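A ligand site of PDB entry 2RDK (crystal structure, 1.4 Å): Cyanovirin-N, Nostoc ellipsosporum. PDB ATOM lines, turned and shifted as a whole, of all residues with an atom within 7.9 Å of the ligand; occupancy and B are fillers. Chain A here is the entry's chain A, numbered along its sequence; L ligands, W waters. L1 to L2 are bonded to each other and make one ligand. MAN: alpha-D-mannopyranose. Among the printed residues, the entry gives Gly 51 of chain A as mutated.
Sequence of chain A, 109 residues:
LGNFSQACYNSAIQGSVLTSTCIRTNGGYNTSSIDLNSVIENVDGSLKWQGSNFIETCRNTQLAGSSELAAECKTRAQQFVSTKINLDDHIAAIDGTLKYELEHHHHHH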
ATOM      1  N   ASN A  37      22.667   5.255 -25.389  1.00  0.00           N
ATOM      2  CA  ASN A  37      22.514   4.191 -24.404  1.00  0.00           C
ATOM      3  C   ASN A  37      22.147   4.694 -23.002  1.00  0.00           C
ATOM      4  O   ASN A  37      21.637   3.944 -22.172  1.00  0.00           O
ATOM      5  CB  ASN A  37      23.775   3.347 -24.363  1.00  0.00           C
ATOM      6  CG  ASN A  37      23.559   2.017 -23.699  1.00  0.00           C
ATOM      7  OD1 ASN A  37      22.564   1.334 -23.960  1.00  0.00           O
ATOM      8  ND2 ASN A  37      24.518   1.589 -22.870  1.00  0.00           N
ATOM      9  N   ILE A  40      17.846   5.330 -23.737  1.00  0.00           N
ATOM     10  CA  ILE A  40      16.951   4.406 -24.422  1.00  0.00           C
ATOM     11  C   ILE A  40      17.108   3.021 -23.806  1.00  0.00           C
ATOM     12  O   ILE A  40      18.235   2.532 -23.602  1.00  0.00           O
ATOM     13  CB  ILE A  40      17.225   4.392 -25.947  1.00  0.00           C
ATOM     14  CG1 ILE A  40      16.902   5.778 -26.543  1.00  0.00           C
ATOM     15  CG2 ILE A  40      16.429   3.308 -26.663  1.00  0.00           C
ATOM     16  CD1 ILE A  40      17.299   5.963 -27.992  1.00  0.00           C
ATOM     17  N   GLU A  41      15.959   2.388 -23.558  1.00  0.00           N
ATOM     18  CA  GLU A  41      15.907   1.062 -22.963  1.00  0.00           C
ATOM     19  C   GLU A  41      15.315   0.061 -23.956  1.00  0.00           C
ATOM     20  O   GLU A  41      14.438   0.401 -24.755  1.00  0.00           O
ATOM     21  CB  GLU A  41      15.047   1.068 -21.686  1.00  0.00           C
ATOM     22  CG  GLU A  41      15.094  -0.239 -20.887  1.00  0.00           C
ATOM     23  CD  GLU A  41      14.142  -0.302 -19.696  1.00  0.00           C
ATOM     24  OE1 GLU A  41      13.588   0.732 -19.295  1.00  0.00           O
ATOM     25  OE2 GLU A  41      13.947  -1.418 -19.166  1.00  0.00           O
ATOM     26  N   ASN A  42      15.829  -1.169 -23.909  1.00  0.00           N
ATOM     27  CA  ASN A  42      15.185  -2.262 -24.612  1.00  0.00           C
ATOM     28  C   ASN A  42      14.159  -2.893 -23.673  1.00  0.00           C
ATOM     29  O   ASN A  42      14.534  -3.559 -22.698  1.00  0.00           O
ATOM     30  CB  ASN A  42      16.225  -3.307 -25.039  1.00  0.00           C
ATOM     31  CG  ASN A  42      15.587  -4.605 -25.528  1.00  0.00           C
ATOM     32  OD1 ASN A  42      14.419  -4.628 -25.906  1.00  0.00           O
ATOM     33  ND2 ASN A  42      16.356  -5.697 -25.510  1.00  0.00           N
ATOM     34  N   VAL A  43      12.873  -2.670 -23.953  1.00  0.00           N
ATOM     35  CA  VAL A  43      11.784  -3.215 -23.145  1.00  0.00           C
ATOM     36  C   VAL A  43      11.115  -4.348 -23.924  1.00  0.00           C
ATOM     37  O   VAL A  43      10.298  -4.115 -24.815  1.00  0.00           O
ATOM     38  CB  VAL A  43      10.767  -2.128 -22.735  1.00  0.00           C
ATOM     39  CG1 VAL A  43       9.698  -2.736 -21.865  1.00  0.00           C
ATOM     40  CG2 VAL A  43      11.438  -0.968 -21.983  1.00  0.00           C
ATOM     41  N   ASP A  44      11.467  -5.597 -23.588  1.00  0.00           N
ATOM     42  CA  ASP A  44      10.891  -6.779 -24.242  1.00  0.00           C
ATOM     43  C   ASP A  44      11.018  -6.756 -25.774  1.00  0.00           C
ATOM     44  O   ASP A  44      10.119  -7.205 -26.487  1.00  0.00           O
ATOM     45  CB  ASP A  44       9.418  -6.964 -23.817  1.00  0.00           C
ATOM     46  CG  ASP A  44       8.903  -8.374 -24.098  1.00  0.00           C
ATOM     47  OD1 ASP A  44       9.690  -9.333 -24.003  1.00  0.00           O
ATOM     48  OD2 ASP A  44       7.699  -8.518 -24.399  1.00  0.00           O
ATOM     49  N   GLY A  45      12.146  -6.255 -26.264  1.00  0.00           N
ATOM     50  CA  GLY A  45      12.424  -6.190 -27.703  1.00  0.00           C
ATOM     51  C   GLY A  45      12.160  -4.850 -28.353  1.00  0.00           C
ATOM     52  O   GLY A  45      12.582  -4.634 -29.483  1.00  0.00           O
ATOM     53  N   SER A  46      11.427  -3.966 -27.670  1.00  0.00           N
ATOM     54  CA  SER A  46      11.089  -2.635 -28.196  1.00  0.00           C
ATOM     55  C   SER A  46      11.925  -1.525 -27.567  1.00  0.00           C
ATOM     56  O   SER A  46      12.011  -1.436 -26.344  1.00  0.00           O
ATOM     57  CB  SER A  46       9.606  -2.330 -27.982  1.00  0.00           C
ATOM     58  OG  SER A  46       8.759  -3.148 -28.776  1.00  0.00           O
ATOM     59  N   LEU A  47      12.465  -0.643 -28.407  1.00  0.00           N
ATOM     60  CA  LEU A  47      13.199   0.533 -27.909  1.00  0.00           C
ATOM     61  C   LEU A  47      12.210   1.552 -27.331  1.00  0.00           C
ATOM     62  O   LEU A  47      11.231   1.919 -27.967  1.00  0.00           O
ATOM     63  CB  LEU A  47      14.011   1.178 -29.020  1.00  0.00           C
ATOM     64  CG  LEU A  47      15.099   0.295 -29.633  1.00  0.00           C
ATOM     65  CD1 LEU A  47      15.625   0.912 -30.930  1.00  0.00           C
ATOM     66  CD2 LEU A  47      16.255   0.017 -28.642  1.00  0.00           C
ATOM     67  N   LYS A  48      12.485   1.993 -26.098  1.00  0.00           N
ATOM     68  CA  LYS A  48      11.649   2.958 -25.400  1.00  0.00           C
ATOM     69  C   LYS A  48      12.504   4.006 -24.709  1.00  0.00           C
ATOM     70  O   LYS A  48      13.655   3.736 -24.358  1.00  0.00           O
ATOM     71  CB  LYS A  48      10.794   2.277 -24.326  1.00  0.00           C
ATOM     72  CG  LYS A  48       9.770   1.285 -24.873  1.00  0.00           C
ATOM     73  CD  LYS A  48       8.617   1.989 -25.572  1.00  0.00           C
ATOM     74  CE  LYS A  48       7.824   1.055 -26.475  1.00  0.00           C
ATOM     75  NZ  LYS A  48       7.031   0.064 -25.694  1.00  0.00           N
ATOM     76  N   GLY A  51      14.549   4.945 -19.855  1.00  0.00           N
ATOM     77  CA  GLY A  51      15.444   3.910 -19.330  1.00  0.00           C
ATOM     78  C   GLY A  51      16.771   3.988 -20.039  1.00  0.00           C
ATOM     79  O   GLY A  51      17.072   4.986 -20.695  1.00  0.00           O
ATOM     80  N   SER A  52      17.563   2.924 -19.913  1.00  0.00           N
ATOM     81  CA  SER A  52      18.931   2.902 -20.429  1.00  0.00           C
ATOM     82  C   SER A  52      19.333   1.487 -20.836  1.00  0.00           C
ATOM     83  O   SER A  52      18.568   0.537 -20.653  1.00  0.00           O
ATOM     84  CB  SER A  52      19.919   3.395 -19.356  1.00  0.00           C
ATOM     85  OG  SER A  52      19.529   4.623 -18.758  1.00  0.00           O
ATOM     86  N   ASN A  53      20.526   1.381 -21.426  1.00  0.00           N
ATOM     87  CA  ASN A  53      21.261   0.131 -21.536  1.00  0.00           C
ATOM     88  C   ASN A  53      20.781  -0.790 -22.669  1.00  0.00           C
ATOM     89  O   ASN A  53      21.126  -1.980 -22.692  1.00  0.00           O
ATOM     90  CB  ASN A  53      21.283  -0.642 -20.198  1.00  0.00           C
ATOM     91  CG  ASN A  53      21.858   0.168 -19.049  1.00  0.00           C
ATOM     92  OD1 ASN A  53      21.284   0.219 -17.940  1.00  0.00           O
ATOM     93  ND2 ASN A  53      22.955   0.849 -19.318  1.00  0.00           N
ATOM     94  N   PHE A  54      20.030  -0.235 -23.624  1.00  0.00           N
ATOM     95  CA  PHE A  54      19.562  -1.053 -24.756  1.00  0.00           C
ATOM     96  C   PHE A  54      20.688  -1.774 -25.504  1.00  0.00           C
ATOM     97  O   PHE A  54      20.511  -2.864 -26.033  1.00  0.00           O
ATOM     98  CB  PHE A  54      18.704  -0.218 -25.730  1.00  0.00           C
ATOM     99  CG  PHE A  54      19.483   0.609 -26.715  1.00  0.00           C
ATOM    100  CD1 PHE A  54      19.778   0.103 -27.985  1.00  0.00           C
ATOM    101  CD2 PHE A  54      19.918   1.893 -26.399  1.00  0.00           C
ATOM    102  CE1 PHE A  54      20.495   0.858 -28.911  1.00  0.00           C
ATOM    103  CE2 PHE A  54      20.638   2.653 -27.317  1.00  0.00           C
ATOM    104  CZ  PHE A  54      20.925   2.144 -28.582  1.00  0.00           C
ATOM    105  N   ILE A  55      21.872  -1.172 -25.523  1.00  0.00           N
ATOM    106  CA  ILE A  55      22.954  -1.678 -26.370  1.00  0.00           C
ATOM    107  C   ILE A  55      23.435  -3.060 -25.900  1.00  0.00           C
ATOM    108  O   ILE A  55      24.027  -3.815 -26.676  1.00  0.00           O
ATOM    109  CB  ILE A  55      24.130  -0.643 -26.500  1.00  0.00           C
ATOM    110  CG1 ILE A  55      24.825  -0.780 -27.864  1.00  0.00           C
ATOM    111  CG2 ILE A  55      25.103  -0.742 -25.331  1.00  0.00           C
ATOM    112  CD1 ILE A  55      23.945  -0.498 -29.092  1.00  0.00           C
ATOM    113  N   GLU A  56      23.161  -3.399 -24.635  1.00  0.00           N
ATOM    114  CA  GLU A  56      23.580  -4.691 -24.086  1.00  0.00           C
ATOM    115  C   GLU A  56      22.833  -5.873 -24.683  1.00  0.00           C
ATOM    116  O   GLU A  56      23.345  -6.993 -24.658  1.00  0.00           O
ATOM    117  CB  GLU A  56      23.349  -4.719 -22.576  1.00  0.00           C
ATOM    118  CG  GLU A  56      24.236  -3.786 -21.787  1.00  0.00           C
ATOM    119  CD  GLU A  56      23.951  -3.846 -20.289  1.00  0.00           C
ATOM    120  OE1 GLU A  56      23.405  -4.854 -19.793  1.00  0.00           O
ATOM    121  OE2 GLU A  56      24.285  -2.865 -19.600  1.00  0.00           O
ATOM    122  N   THR A  57      21.623  -5.630 -25.189  1.00  0.00           N
ATOM    123  CA  THR A  57      20.739  -6.700 -25.634  1.00  0.00           C
ATOM    124  C   THR A  57      20.132  -6.393 -27.001  1.00  0.00           C
ATOM    125  O   THR A  57      19.101  -6.971 -27.376  1.00  0.00           O
ATOM    126  CB  THR A  57      19.619  -6.957 -24.603  1.00  0.00           C
ATOM    127  OG1 THR A  57      18.919  -5.739 -24.334  1.00  0.00           O
ATOM    128  CG2 THR A  57      20.193  -7.560 -23.315  1.00  0.00           C
ATOM    129  N   CYS A  58      20.781  -5.501 -27.741  1.00  0.00           N
ATOM    130  CA  CYS A  58      20.399  -5.208 -29.117  1.00  0.00           C
ATOM    131  C   CYS A  58      21.620  -5.329 -30.027  1.00  0.00           C
ATOM    132  O   CYS A  58      22.758  -5.350 -29.557  1.00  0.00           O
ATOM    133  CB  CYS A  58      19.763  -3.808 -29.238  1.00  0.00           C
ATOM    134  SG  CYS A  58      18.301  -3.485 -28.201  1.00  0.00           S
ATOM    135  N   CYS A  73      16.494  -6.222 -31.313  1.00  0.00           N
ATOM    136  CA  CYS A  73      16.594  -6.343 -29.864  1.00  0.00           C
ATOM    137  C   CYS A  73      15.980  -7.633 -29.326  1.00  0.00           C
ATOM    138  O   CYS A  73      15.000  -8.151 -29.879  1.00  0.00           O
ATOM    139  CB  CYS A  73      15.923  -5.164 -29.182  1.00  0.00           C
ATOM    140  SG  CYS A  73      16.702  -3.566 -29.467  1.00  0.00           S
ATOM    141  N   LYS A  74      16.555  -8.127 -28.237  1.00  0.00           N
ATOM    142  CA  LYS A  74      16.091  -9.355 -27.617  1.00  0.00           C
ATOM    143  C   LYS A  74      14.870  -9.100 -26.731  1.00  0.00           C
ATOM    144  O   LYS A  74      14.853  -8.178 -25.917  1.00  0.00           O
ATOM    145  CB  LYS A  74      17.187  -9.982 -26.750  1.00  0.00           C
ATOM    146  CG  LYS A  74      18.314 -10.609 -27.501  1.00  0.00           C
ATOM    147  CD  LYS A  74      19.088 -11.603 -26.614  1.00  0.00           C
ATOM    148  CE  LYS A  74      19.684 -10.935 -25.362  1.00  0.00           C
ATOM    149  NZ  LYS A  74      20.607 -11.845 -24.630  1.00  0.00           N
ATOM    150  N   THR A  75      13.869  -9.958 -26.872  1.00  0.00           N
ATOM    151  CA  THR A  75      12.734  -9.981 -25.961  1.00  0.00           C
ATOM    152  C   THR A  75      13.145 -10.617 -24.625  1.00  0.00           C
ATOM    153  O   THR A  75      14.239 -11.181 -24.512  1.00  0.00           O
ATOM    154  CB  THR A  75      11.610 -10.824 -26.578  1.00  0.00           C
ATOM    155  OG1 THR A  75      12.068 -12.190 -26.663  1.00  0.00           O
ATOM    156  CG2 THR A  75      11.241 -10.297 -27.953  1.00  0.00           C
ATOM    157  N   ARG A  76      12.274 -10.564 -23.630  1.00  0.00           N
ATOM    158  CA  ARG A  76      12.543 -11.229 -22.360  1.00  0.00           C
ATOM    159  C   ARG A  76      12.762 -12.732 -22.541  1.00  0.00           C
ATOM    160  O   ARG A  76      13.573 -13.334 -21.841  1.00  0.00           O
ATOM    161  CB  ARG A  76      11.447 -10.949 -21.329  1.00  0.00           C
ATOM    162  CG  ARG A  76      11.504  -9.526 -20.784  1.00  0.00           C
ATOM    163  CD  ARG A  76      10.518  -9.306 -19.650  1.00  0.00           C
ATOM    164  NE  ARG A  76       9.129  -9.267 -20.093  1.00  0.00           N
ATOM    165  CZ  ARG A  76       8.416  -8.156 -20.306  1.00  0.00           C
ATOM    166  NH1 ARG A  76       8.968  -6.963 -20.122  1.00  0.00           N
ATOM    167  NH2 ARG A  76       7.155  -8.252 -20.685  1.00  0.00           N
ATOM    168  N   ALA A  77      12.058 -13.310 -23.511  1.00  0.00           N
ATOM    169  CA  ALA A  77      12.212 -14.723 -23.871  1.00  0.00           C
ATOM    170  C   ALA A  77      13.424 -15.018 -24.757  1.00  0.00           C
ATOM    171  O   ALA A  77      13.614 -16.151 -25.221  1.00  0.00           O
ATOM    172  CB  ALA A  77      10.936 -15.222 -24.526  1.00  0.00           C
ATOM    173  N   GLN A  78      14.261 -13.996 -24.979  1.00  0.00           N
ATOM    174  CA  GLN A  78      15.579 -14.166 -25.600  1.00  0.00           C
ATOM    175  C   GLN A  78      15.545 -14.421 -27.107  1.00  0.00           C
ATOM    176  O   GLN A  78      16.426 -15.082 -27.651  1.00  0.00           O
ATOM    177  CB  GLN A  78      16.400 -15.263 -24.875  1.00  0.00           C
ATOM    178  CG  GLN A  78      16.542 -15.023 -23.373  1.00  0.00           C
ATOM    179  CD  GLN A  78      17.187 -13.677 -23.066  1.00  0.00           C
ATOM    180  OE1 GLN A  78      16.547 -12.772 -22.531  1.00  0.00           O
ATOM    181  NE2 GLN A  78      18.447 -13.537 -23.431  1.00  0.00           N
ATOM    182  N   GLN A  79      14.535 -13.864 -27.764  1.00  0.00           N
ATOM    183  CA  GLN A  79      14.489 -13.922 -29.230  1.00  0.00           C
ATOM    184  C   GLN A  79      14.533 -12.511 -29.808  1.00  0.00           C
ATOM    185  O   GLN A  79      14.145 -11.534 -29.148  1.00  0.00           O
ATOM    186  CB  GLN A  79      13.261 -14.697 -29.730  1.00  0.00           C
ATOM    187  CG  GLN A  79      13.199 -16.162 -29.247  1.00  0.00           C
ATOM    188  CD  GLN A  79      12.083 -16.936 -29.914  1.00  0.00           C
ATOM    189  OE1 GLN A  79      11.377 -16.425 -30.791  1.00  0.00           O
ATOM    190  NE2 GLN A  79      11.919 -18.201 -29.516  1.00  0.00           N
HETATM  191  C1  MAN L   1      16.084  -7.693 -19.710  1.00  0.00           C
HETATM  192  C2  MAN L   1      15.225  -6.451 -20.004  1.00  0.00           C
HETATM  193  C3  MAN L   1      14.210  -6.760 -21.119  1.00  0.00           C
HETATM  194  C4  MAN L   1      14.883  -7.348 -22.353  1.00  0.00           C
HETATM  195  C5  MAN L   1      15.802  -8.517 -21.941  1.00  0.00           C
HETATM  196  C6  MAN L   1      16.619  -8.994 -23.141  1.00  0.00           C
HETATM  197  O1  MAN L   1      15.300  -8.728 -19.168  1.00  0.00           O
HETATM  198  O2  MAN L   1      15.991  -5.361 -20.498  1.00  0.00           O
HETATM  199  O3  MAN L   1      13.476  -5.604 -21.478  1.00  0.00           O
HETATM  200  O4  MAN L   1      13.885  -7.759 -23.277  1.00  0.00           O
HETATM  201  O5  MAN L   1      16.700  -8.134 -20.909  1.00  0.00           O
HETATM  202  O6  MAN L   1      17.488 -10.022 -22.729  1.00  0.00           O
HETATM  203  C1  MAN L   2      16.657  -4.568 -19.501  1.00  0.00           C
HETATM  204  C2  MAN L   2      16.800  -3.183 -20.134  1.00  0.00           C
HETATM  205  C3  MAN L   2      17.699  -3.271 -21.368  1.00  0.00           C
HETATM  206  C4  MAN L   2      19.029  -3.938 -21.031  1.00  0.00           C
HETATM  207  C5  MAN L   2      18.800  -5.261 -20.296  1.00  0.00           C
HETATM  208  C6  MAN L   2      20.114  -5.873 -19.817  1.00  0.00           C
HETATM  209  O2  MAN L   2      17.329  -2.285 -19.171  1.00  0.00           O
HETATM  210  O3  MAN L   2      17.881  -1.989 -21.947  1.00  0.00           O
HETATM  211  O4  MAN L   2      19.750  -4.166 -22.225  1.00  0.00           O
HETATM  212  O5  MAN L   2      17.937  -5.074 -19.174  1.00  0.00           O
HETATM  213  O6  MAN L   2      19.913  -7.191 -19.342  1.00  0.00           O
HETATM  214  O   HOH W   1      19.448  -2.257 -17.530  1.00  0.00           O
HETATM  215  O   HOH W   2      11.435  -5.598 -19.524  1.00  0.00           O
HETATM  216  O   HOH W   3      13.309 -10.418 -17.212  1.00  0.00           O
HETATM  217  O   HOH W   4      19.394  -9.691 -20.683  1.00  0.00           O
HETATM  218  O   HOH W   5      23.147  -7.456 -19.974  1.00  0.00           O
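The backbone NH (N) of Asn 42 is in hydrogen-bond range of an oxygen (O3) of MAN L2 (3.0 Å).
The backbone carbonyl oxygen (O) of Asn 53 sits at hydrogen-bond distance from an oxygen (O4) of MAN L2.
An oxygen (O6) of MAN L1 lies within hydrogen-bond range of the side-chain amide oxygen of Gln 78 (2.9 Å).
An oxygen (O3) of MAN L2 sits at hydrogen-bond distance from the backbone carbonyl oxygen (O) of Ser 52 (2.9 Å).
The backbone carbonyl oxygen of Asn 42 is in hydrogen-bond range of an oxygen (O3) of MAN L1, 2.6 Å away.
An oxygen (O4) of MAN L2 lies within hydrogen-bond range of the side-chain hydroxyl (OG1) of Thr 57.
The backbone NH of Phe 54 lies within hydrogen-bond range of an oxygen (O3) of MAN L2 (3.2 Å).
An oxygen (O2) of MAN L2 lies close to the side-chain carboxylate (OE2) of Glu 41 (3.5 Å).
O3 of MAN L1 sits at hydrogen-bond distance from N of Asp 44 (2.9 Å).
N of Arg 76 lies within hydrogen-bond range of O4 of MAN L1 (3.3 Å).
O of Lys 74 sits at hydrogen-bond distance from O4 of MAN L1 (2.8 Å).
The backbone carbonyl oxygen of Lys 74 sits at hydrogen-bond distance from the backbone NH of Gly 45 (3.3 Å).
OD1 of Asn 42 sits at hydrogen-bond distance from N of Gly 45.
The backbone carbonyl oxygen (O) of Ile 40 sits at hydrogen-bond distance from the backbone NH (N) of Phe 54.
N of Asn 53 sits at hydrogen-bond distance from O of Asn 37, 2.9 Å away.
The backbone NH (N) of Glu 41 sits at hydrogen-bond distance from the backbone carbonyl oxygen (O) of Lys 48 (2.8 Å).
The side-chain amide nitrogen (ND2) of Asn 42 is in hydrogen-bond range of the side-chain hydroxyl (OG1) of Thr 57 (2.8 Å).
OE1 of Gln 78 lies close to O of Arg 76 (3.1 Å).
The backbone NH (N) of Asn 53 is in hydrogen-bond range of the backbone carbonyl oxygen (O) of Ile 40 (3.4 Å).
Residues that only touch the ligand: Val 43 (3.4 Å), Gly 45 (3.8 Å), Glu 56 (3.4 Å) and Thr 75 (3.2 Å).
Water W1 bridges O2 of MAN L2 and OD1 of Asn 53.
Water W2 lies within hydrogen-bond range of O3 of MAN L1 (2.8 Å) and NH1 of Arg 76 (2.9 Å).
Water W5 lies within hydrogen-bond range of OE1 of Glu 56 (2.6 Å) and O6 of MAN L2 (3.3 Å).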
